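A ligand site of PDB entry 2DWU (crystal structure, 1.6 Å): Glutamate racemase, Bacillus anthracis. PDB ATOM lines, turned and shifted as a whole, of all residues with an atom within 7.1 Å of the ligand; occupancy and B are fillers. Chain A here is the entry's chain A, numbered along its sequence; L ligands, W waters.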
ATOM      1  N   ASP A  14     -33.730  -9.235 -24.132  1.00  0.00           N
ATOM      2  CA  ASP A  14     -33.231 -10.301 -23.261  1.00  0.00           C
ATOM      3  C   ASP A  14     -33.219 -11.589 -24.050  1.00  0.00           C
ATOM      4  O   ASP A  14     -33.806 -11.649 -25.108  1.00  0.00           O
ATOM      5  CB  ASP A  14     -34.164 -10.467 -22.055  1.00  0.00           C
ATOM      6  CG  ASP A  14     -33.687 -11.562 -21.104  1.00  0.00           C
ATOM      7  OD1 ASP A  14     -32.514 -11.500 -20.659  1.00  0.00           O
ATOM      8  OD2 ASP A  14     -34.464 -12.496 -20.812  1.00  0.00           O
ATOM      9  N   SER A  15     -32.542 -12.616 -23.537  1.00  0.00           N
ATOM     10  CA  SER A  15     -32.547 -13.882 -24.230  1.00  0.00           C
ATOM     11  C   SER A  15     -33.883 -14.629 -24.103  1.00  0.00           C
ATOM     12  O   SER A  15     -34.127 -15.555 -24.865  1.00  0.00           O
ATOM     13  CB  SER A  15     -31.422 -14.759 -23.692  1.00  0.00           C
ATOM     14  OG  SER A  15     -31.667 -15.099 -22.344  1.00  0.00           O
ATOM     15  N   GLY A  16     -34.739 -14.243 -23.149  1.00  0.00           N
ATOM     16  CA  GLY A  16     -36.005 -14.940 -22.970  1.00  0.00           C
ATOM     17  C   GLY A  16     -36.950 -14.292 -21.961  1.00  0.00           C
ATOM     18  O   GLY A  16     -37.322 -13.128 -22.129  1.00  0.00           O
ATOM     19  N   VAL A  17     -37.329 -15.045 -20.932  1.00  0.00           N
ATOM     20  CA  VAL A  17     -38.223 -14.548 -19.890  1.00  0.00           C
ATOM     21  C   VAL A  17     -37.487 -13.948 -18.692  1.00  0.00           C
ATOM     22  O   VAL A  17     -38.048 -13.139 -17.953  1.00  0.00           O
ATOM     23  CB  VAL A  17     -39.159 -15.670 -19.343  1.00  0.00           C
ATOM     24  CG1 VAL A  17     -40.217 -16.014 -20.349  1.00  0.00           C
ATOM     25  CG2 VAL A  17     -38.365 -16.916 -18.971  1.00  0.00           C
ATOM     26  N   GLY A  18     -36.225 -14.322 -18.514  1.00  0.00           N
ATOM     27  CA  GLY A  18     -35.464 -13.829 -17.371  1.00  0.00           C
ATOM     28  C   GLY A  18     -35.492 -12.329 -17.212  1.00  0.00           C
ATOM     29  O   GLY A  18     -35.618 -11.811 -16.091  1.00  0.00           O
ATOM     30  N   GLY A  19     -35.390 -11.622 -18.337  1.00  0.00           N
ATOM     31  CA  GLY A  19     -35.384 -10.173 -18.339  1.00  0.00           C
ATOM     32  C   GLY A  19     -36.625  -9.529 -17.733  1.00  0.00           C
ATOM     33  O   GLY A  19     -36.663  -8.308 -17.545  1.00  0.00           O
ATOM     34  N   ARG A  43     -34.074 -19.032 -28.932  1.00  0.00           N
ATOM     35  CA  ARG A  43     -32.638 -19.302 -28.917  1.00  0.00           C
ATOM     36  C   ARG A  43     -32.004 -19.235 -27.534  1.00  0.00           C
ATOM     37  O   ARG A  43     -30.789 -19.177 -27.401  1.00  0.00           O
ATOM     38  CB  ARG A  43     -31.916 -18.385 -29.904  1.00  0.00           C
ATOM     39  CG  ARG A  43     -32.467 -18.573 -31.338  1.00  0.00           C
ATOM     40  CD  ARG A  43     -31.726 -17.770 -32.407  1.00  0.00           C
ATOM     41  NE  ARG A  43     -31.914 -16.336 -32.257  1.00  0.00           N
ATOM     42  CZ  ARG A  43     -31.783 -15.455 -33.246  1.00  0.00           C
ATOM     43  NH1 ARG A  43     -31.444 -15.853 -34.461  1.00  0.00           N
ATOM     44  NH2 ARG A  43     -31.960 -14.149 -33.005  1.00  0.00           N
ATOM     45  N   CYS A  44     -32.845 -19.189 -26.512  1.00  0.00           N
ATOM     46  CA  CYS A  44     -32.390 -19.175 -25.121  1.00  0.00           C
ATOM     47  C   CYS A  44     -31.986 -20.636 -24.840  1.00  0.00           C
ATOM     48  O   CYS A  44     -32.686 -21.571 -25.254  1.00  0.00           O
ATOM     49  CB  CYS A  44     -33.553 -18.739 -24.227  1.00  0.00           C
ATOM     50  SG  CYS A  44     -33.135 -18.442 -22.500  1.00  0.00           S
ATOM     51  N   PRO A  45     -30.899 -20.872 -24.079  1.00  0.00           N
ATOM     52  CA  PRO A  45     -30.011 -19.891 -23.440  1.00  0.00           C
ATOM     53  C   PRO A  45     -28.871 -19.329 -24.244  1.00  0.00           C
ATOM     54  O   PRO A  45     -28.328 -19.987 -25.145  1.00  0.00           O
ATOM     55  CB  PRO A  45     -29.495 -20.666 -22.226  1.00  0.00           C
ATOM     56  CG  PRO A  45     -29.314 -22.041 -22.804  1.00  0.00           C
ATOM     57  CD  PRO A  45     -30.578 -22.233 -23.621  1.00  0.00           C
ATOM     58  N   TYR A  46     -28.470 -18.111 -23.884  1.00  0.00           N
ATOM     59  CA  TYR A  46     -27.320 -17.450 -24.490  1.00  0.00           C
ATOM     60  C   TYR A  46     -26.041 -17.784 -23.686  1.00  0.00           C
ATOM     61  O   TYR A  46     -24.918 -17.717 -24.216  1.00  0.00           O
ATOM     62  CB  TYR A  46     -27.507 -15.932 -24.451  1.00  0.00           C
ATOM     63  CG  TYR A  46     -28.432 -15.358 -25.499  1.00  0.00           C
ATOM     64  CD1 TYR A  46     -29.209 -16.191 -26.333  1.00  0.00           C
ATOM     65  CD2 TYR A  46     -28.514 -13.985 -25.662  1.00  0.00           C
ATOM     66  CE1 TYR A  46     -30.040 -15.619 -27.322  1.00  0.00           C
ATOM     67  CE2 TYR A  46     -29.326 -13.417 -26.625  1.00  0.00           C
ATOM     68  CZ  TYR A  46     -30.080 -14.234 -27.446  1.00  0.00           C
ATOM     69  OH  TYR A  46     -30.864 -13.619 -28.390  1.00  0.00           O
ATOM     70  N   GLY A  47     -26.221 -18.152 -22.423  1.00  0.00           N
ATOM     71  CA  GLY A  47     -25.086 -18.408 -21.557  1.00  0.00           C
ATOM     72  C   GLY A  47     -23.960 -19.268 -22.123  1.00  0.00           C
ATOM     73  O   GLY A  47     -22.793 -18.891 -22.006  1.00  0.00           O
ATOM     74  N   PRO A  48     -24.288 -20.412 -22.747  1.00  0.00           N
ATOM     75  CA  PRO A  48     -23.287 -21.308 -23.331  1.00  0.00           C
ATOM     76  C   PRO A  48     -22.889 -21.028 -24.772  1.00  0.00           C
ATOM     77  O   PRO A  48     -22.069 -21.761 -25.350  1.00  0.00           O
ATOM     78  CB  PRO A  48     -23.956 -22.686 -23.218  1.00  0.00           C
ATOM     79  CG  PRO A  48     -25.132 -22.482 -22.276  1.00  0.00           C
ATOM     80  CD  PRO A  48     -25.584 -21.089 -22.618  1.00  0.00           C
ATOM     81  N   ALA A  76     -31.168  -6.152 -20.929  1.00  0.00           N
ATOM     82  CA  ALA A  76     -31.521  -6.764 -19.657  1.00  0.00           C
ATOM     83  C   ALA A  76     -30.768  -8.054 -19.345  1.00  0.00           C
ATOM     84  O   ALA A  76     -30.644  -8.435 -18.174  1.00  0.00           O
ATOM     85  CB  ALA A  76     -33.037  -7.017 -19.616  1.00  0.00           C
ATOM     86  N   CYS A  77     -30.257  -8.709 -20.382  1.00  0.00           N
ATOM     87  CA  CYS A  77     -29.560  -9.977 -20.234  1.00  0.00           C
ATOM     88  C   CYS A  77     -28.075  -9.754 -19.913  1.00  0.00           C
ATOM     89  O   CYS A  77     -27.392  -9.079 -20.670  1.00  0.00           O
ATOM     90  CB  CYS A  77     -29.726 -10.760 -21.534  1.00  0.00           C
ATOM     91  SG  CYS A  77     -28.815 -12.309 -21.635  1.00  0.00           S
ATOM     92  N   ASN A  78     -27.591 -10.328 -18.809  1.00  0.00           N
ATOM     93  CA  ASN A  78     -26.186 -10.110 -18.443  1.00  0.00           C
ATOM     94  C   ASN A  78     -25.255 -10.738 -19.484  1.00  0.00           C
ATOM     95  O   ASN A  78     -24.182 -10.191 -19.761  1.00  0.00           O
ATOM     96  CB  ASN A  78     -25.897 -10.703 -17.050  1.00  0.00           C
ATOM     97  CG  ASN A  78     -26.691 -10.021 -15.946  1.00  0.00           C
ATOM     98  OD1 ASN A  78     -26.161  -9.211 -15.132  1.00  0.00           O
ATOM     99  ND2 ASN A  78     -27.962 -10.313 -15.900  1.00  0.00           N
ATOM    100  N   THR A  79     -25.650 -11.882 -20.014  1.00  0.00           N
ATOM    101  CA  THR A  79     -24.843 -12.589 -21.025  1.00  0.00           C
ATOM    102  C   THR A  79     -24.751 -11.749 -22.302  1.00  0.00           C
ATOM    103  O   THR A  79     -23.674 -11.608 -22.929  1.00  0.00           O
ATOM    104  CB  THR A  79     -25.456 -13.965 -21.379  1.00  0.00           C
ATOM    105  OG1 THR A  79     -25.538 -14.774 -20.188  1.00  0.00           O
ATOM    106  CG2 THR A  79     -24.619 -14.662 -22.423  1.00  0.00           C
ATOM    107  N   ALA A  80     -25.888 -11.192 -22.710  1.00  0.00           N
ATOM    108  CA  ALA A  80     -25.908 -10.358 -23.904  1.00  0.00           C
ATOM    109  C   ALA A  80     -25.119  -9.076 -23.662  1.00  0.00           C
ATOM    110  O   ALA A  80     -24.401  -8.608 -24.542  1.00  0.00           O
ATOM    111  CB  ALA A  80     -27.367 -10.042 -24.272  1.00  0.00           C
ATOM    112  N   VAL A  99     -26.928  -4.262 -17.938  1.00  0.00           N
ATOM    113  CA  VAL A  99     -27.162  -4.634 -16.540  1.00  0.00           C
ATOM    114  C   VAL A  99     -25.921  -4.899 -15.714  1.00  0.00           C
ATOM    115  O   VAL A  99     -26.031  -5.066 -14.506  1.00  0.00           O
ATOM    116  CB  VAL A  99     -28.058  -5.901 -16.434  1.00  0.00           C
ATOM    117  CG1 VAL A  99     -29.514  -5.522 -16.750  1.00  0.00           C
ATOM    118  CG2 VAL A  99     -27.601  -6.979 -17.439  1.00  0.00           C
ATOM    119  N   GLY A 120     -22.841 -15.748 -12.456  1.00  0.00           N
ATOM    120  CA  GLY A 120     -23.583 -15.561 -13.679  1.00  0.00           C
ATOM    121  C   GLY A 120     -23.324 -16.733 -14.593  1.00  0.00           C
ATOM    122  O   GLY A 120     -22.748 -17.748 -14.192  1.00  0.00           O
ATOM    123  N   THR A 121     -23.733 -16.598 -15.845  1.00  0.00           N
ATOM    124  CA  THR A 121     -23.519 -17.679 -16.808  1.00  0.00           C
ATOM    125  C   THR A 121     -22.045 -17.762 -17.197  1.00  0.00           C
ATOM    126  O   THR A 121     -21.244 -16.865 -16.927  1.00  0.00           O
ATOM    127  CB  THR A 121     -24.282 -17.407 -18.146  1.00  0.00           C
ATOM    128  OG1 THR A 121     -23.728 -16.216 -18.745  1.00  0.00           O
ATOM    129  CG2 THR A 121     -25.791 -17.236 -17.913  1.00  0.00           C
ATOM    130  N   THR A 124     -21.072 -14.799 -19.268  1.00  0.00           N
ATOM    131  CA  THR A 124     -20.896 -13.579 -18.504  1.00  0.00           C
ATOM    132  C   THR A 124     -19.583 -13.564 -17.745  1.00  0.00           C
ATOM    133  O   THR A 124     -18.853 -12.571 -17.776  1.00  0.00           O
ATOM    134  CB  THR A 124     -22.054 -13.400 -17.522  1.00  0.00           C
ATOM    135  OG1 THR A 124     -23.245 -13.185 -18.289  1.00  0.00           O
ATOM    136  CG2 THR A 124     -21.811 -12.163 -16.599  1.00  0.00           C
ATOM    137  N   ALA A 152     -29.920 -20.832 -13.926  1.00  0.00           N
ATOM    138  CA  ALA A 152     -31.026 -20.255 -14.701  1.00  0.00           C
ATOM    139  C   ALA A 152     -32.032 -21.341 -15.101  1.00  0.00           C
ATOM    140  O   ALA A 152     -33.249 -21.134 -15.000  1.00  0.00           O
ATOM    141  CB  ALA A 152     -30.501 -19.505 -15.948  1.00  0.00           C
ATOM    142  N   THR A 153     -31.544 -22.510 -15.519  1.00  0.00           N
ATOM    143  CA  THR A 153     -32.463 -23.596 -15.882  1.00  0.00           C
ATOM    144  C   THR A 153     -33.261 -24.035 -14.657  1.00  0.00           C
ATOM    145  O   THR A 153     -34.467 -24.327 -14.778  1.00  0.00           O
ATOM    146  CB  THR A 153     -31.710 -24.809 -16.471  1.00  0.00           C
ATOM    147  OG1 THR A 153     -30.868 -24.360 -17.544  1.00  0.00           O
ATOM    148  CG2 THR A 153     -32.701 -25.811 -17.039  1.00  0.00           C
ATOM    149  N   GLU A 156     -36.114 -21.670 -14.240  1.00  0.00           N
ATOM    150  CA  GLU A 156     -37.194 -21.814 -15.222  1.00  0.00           C
ATOM    151  C   GLU A 156     -37.955 -23.128 -15.192  1.00  0.00           C
ATOM    152  O   GLU A 156     -39.153 -23.161 -15.494  1.00  0.00           O
ATOM    153  CB  GLU A 156     -36.650 -21.624 -16.633  1.00  0.00           C
ATOM    154  CG  GLU A 156     -36.503 -20.186 -17.008  1.00  0.00           C
ATOM    155  CD  GLU A 156     -36.307 -19.965 -18.486  1.00  0.00           C
ATOM    156  OE1 GLU A 156     -37.033 -20.587 -19.296  1.00  0.00           O
ATOM    157  OE2 GLU A 156     -35.431 -19.160 -18.853  1.00  0.00           O
ATOM    158  N   GLY A 187     -25.326 -11.617 -11.124  1.00  0.00           N
ATOM    159  CA  GLY A 187     -25.059 -11.279 -12.508  1.00  0.00           C
ATOM    160  C   GLY A 187     -25.777 -12.080 -13.576  1.00  0.00           C
ATOM    161  O   GLY A 187     -25.189 -12.443 -14.587  1.00  0.00           O
ATOM    162  N   CYS A 188     -27.063 -12.326 -13.341  1.00  0.00           N
ATOM    163  CA  CYS A 188     -27.910 -13.087 -14.250  1.00  0.00           C
ATOM    164  C   CYS A 188     -29.369 -12.689 -13.984  1.00  0.00           C
ATOM    165  O   CYS A 188     -29.775 -12.527 -12.827  1.00  0.00           O
ATOM    166  CB  CYS A 188     -27.719 -14.576 -14.019  1.00  0.00           C
ATOM    167  SG  CYS A 188     -28.819 -15.657 -15.021  1.00  0.00           S
ATOM    168  N   THR A 189     -30.146 -12.572 -15.059  1.00  0.00           N
ATOM    169  CA  THR A 189     -31.546 -12.189 -14.955  1.00  0.00           C
ATOM    170  C   THR A 189     -32.385 -13.060 -14.039  1.00  0.00           C
ATOM    171  O   THR A 189     -33.352 -12.577 -13.441  1.00  0.00           O
ATOM    172  CB  THR A 189     -32.266 -12.264 -16.343  1.00  0.00           C
ATOM    173  OG1 THR A 189     -31.956 -13.511 -16.973  1.00  0.00           O
ATOM    174  CG2 THR A 189     -31.830 -11.150 -17.269  1.00  0.00           C
ATOM    175  N   HIS A 190     -32.053 -14.344 -13.942  1.00  0.00           N
ATOM    176  CA  HIS A 190     -32.854 -15.272 -13.179  1.00  0.00           C
ATOM    177  C   HIS A 190     -32.594 -15.348 -11.684  1.00  0.00           C
ATOM    178  O   HIS A 190     -33.468 -15.804 -10.917  1.00  0.00           O
ATOM    179  CB  HIS A 190     -32.657 -16.680 -13.760  1.00  0.00           C
ATOM    180  CG  HIS A 190     -33.185 -16.861 -15.149  1.00  0.00           C
ATOM    181  ND1 HIS A 190     -32.823 -16.058 -16.202  1.00  0.00           N
ATOM    182  CD2 HIS A 190     -33.985 -17.826 -15.665  1.00  0.00           C
ATOM    183  CE1 HIS A 190     -33.369 -16.528 -17.324  1.00  0.00           C
ATOM    184  NE2 HIS A 190     -34.079 -17.605 -17.014  1.00  0.00           N
ATOM    185  N   TYR A 191     -31.429 -14.890 -11.248  1.00  0.00           N
ATOM    186  CA  TYR A 191     -31.071 -15.071  -9.851  1.00  0.00           C
ATOM    187  C   TYR A 191     -31.908 -14.399  -8.786  1.00  0.00           C
ATOM    188  O   TYR A 191     -31.938 -14.897  -7.672  1.00  0.00           O
ATOM    189  CB  TYR A 191     -29.571 -14.792  -9.653  1.00  0.00           C
ATOM    190  CG  TYR A 191     -28.648 -15.695 -10.486  1.00  0.00           C
ATOM    191  CD1 TYR A 191     -29.137 -16.762 -11.268  1.00  0.00           C
ATOM    192  CD2 TYR A 191     -27.281 -15.418 -10.546  1.00  0.00           C
ATOM    193  CE1 TYR A 191     -28.282 -17.518 -12.090  1.00  0.00           C
ATOM    194  CE2 TYR A 191     -26.418 -16.155 -11.361  1.00  0.00           C
ATOM    195  CZ  TYR A 191     -26.916 -17.199 -12.124  1.00  0.00           C
ATOM    196  OH  TYR A 191     -26.045 -17.832 -12.951  1.00  0.00           O
HETATM  197  N1  LIG L   1     -30.683 -13.886 -19.485  1.00  0.00           N
HETATM  198  C1  LIG L   1     -29.414 -14.653 -19.232  1.00  0.00           C
HETATM  199  C2  LIG L   1     -28.472 -13.844 -18.397  1.00  0.00           C
HETATM  200  O1  LIG L   1     -27.265 -14.128 -18.303  1.00  0.00           O
HETATM  201  C3  LIG L   1     -29.734 -15.976 -18.517  1.00  0.00           C
HETATM  202  C4  LIG L   1     -30.321 -16.953 -19.552  1.00  0.00           C
HETATM  203  C5  LIG L   1     -29.499 -17.247 -20.724  1.00  0.00           C
HETATM  204  O2  LIG L   1     -29.759 -16.778 -21.830  1.00  0.00           O
HETATM  205  O3  LIG L   1     -28.431 -18.027 -20.543  1.00  0.00           O
HETATM  206  O4  LIG L   1     -28.986 -12.815 -17.742  1.00  0.00           O
HETATM  207  O   HOH W   1     -33.482 -14.935 -20.132  1.00  0.00           O
HETATM  208  O   HOH W   2     -25.269 -14.149 -16.616  1.00  0.00           O
HETATM  209  O   HOH W   3     -28.235 -20.059 -18.977  1.00  0.00           O
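The side-chain hydroxyl (OG) of Ser 15 is in hydrogen-bond range of an oxygen (O2) of the ligand, 2.6 Å away.
The side-chain sulfur of Cys 77 lies within hydrogen-bond range of a nitrogen (N1) of the ligand, 3.3 Å away.
N1 of the ligand is in hydrogen-bond range of OG1 of Thr 189 (2.8 Å).
An oxygen (O3) of the ligand sits at hydrogen-bond distance from the backbone NH (N) of Gly 47.
The backbone NH (N) of Thr 189 is in hydrogen-bond range of an oxygen (O4) of the ligand (2.9 Å).
An oxygen (O1) of the ligand sits at hydrogen-bond distance from the side-chain hydroxyl (OG1) of Thr 79, 2.6 Å away.
ND2 of Asn 78 sits at hydrogen-bond distance from O4 of the ligand, 3.3 Å away.
O4 of the ligand sits at hydrogen-bond distance from N of Asn 78.
A nitrogen (N1) of the ligand is in salt-bridge range of the side-chain carboxylate of Asp 14.
An oxygen (O2) of the ligand is in hydrogen-bond range of the backbone NH (N) of Tyr 46 (2.8 Å).
The backbone NH (N) of Thr 79 is in hydrogen-bond range of an oxygen (O1) of the ligand (3.3 Å).
The side-chain amide nitrogen (ND2) of Asn 78 lies close to the backbone NH (N) of Thr 189, 3.3 Å away.
The side-chain hydroxyl of Ser 15 lies within hydrogen-bond range of the side-chain sulfur of Cys 44.
The side-chain hydroxyl of Thr 79 is in hydrogen-bond range of the side-chain hydroxyl of Thr 121 (2.7 Å).
N of Thr 79 sits close to OG1 of Thr 124, at 3.2 Å.
The backbone NH (N) of Thr 79 sits close to the side-chain sulfur (SG) of Cys 77.
OD2 of Asp 14 sits at hydrogen-bond distance from N of Gly 16, 2.9 Å away.
OD2 of Asp 14 lies within hydrogen-bond range of N of Gly 18, at 3.4 Å.
N of Ala 80 lies within hydrogen-bond range of SG of Cys 77 (3.3 Å).
Cys 44 touches the ligand (SG to O2, 3.8 Å).
CB of Pro 45 touches O3 of the ligand (3.3 Å).
Thr 121 touches the ligand (CG2 to O1, 3.5 Å).
Cys 188 touches the ligand (SG to C3, 3.6 Å).
His 190 touches the ligand (CE1 to C4, 3.8 Å).
Hydrophobic or aromatic side chains that line the ligand: Pro 45, Tyr 46 and His 190.
Within 4 Å of the ligand: Asp 14, Ser 15, Cys 44, Pro 45, Tyr 46, Gly 47, Cys 77, Asn 78, Thr 79, Thr 121, Cys 188, Thr 189 and His 190.
Water W2 lies within hydrogen-bond range of an oxygen (O1) of the ligand, the backbone carbonyl oxygen (O) of Gly 187, the side-chain hydroxyl (OG1) of Thr 124 and the backbone NH (N) of Thr 121.
Water W1 lies within hydrogen-bond range of OD2 of Asp 14, OG of Ser 15, N1 of the ligand, N of Gly 18 and N of Gly 16.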
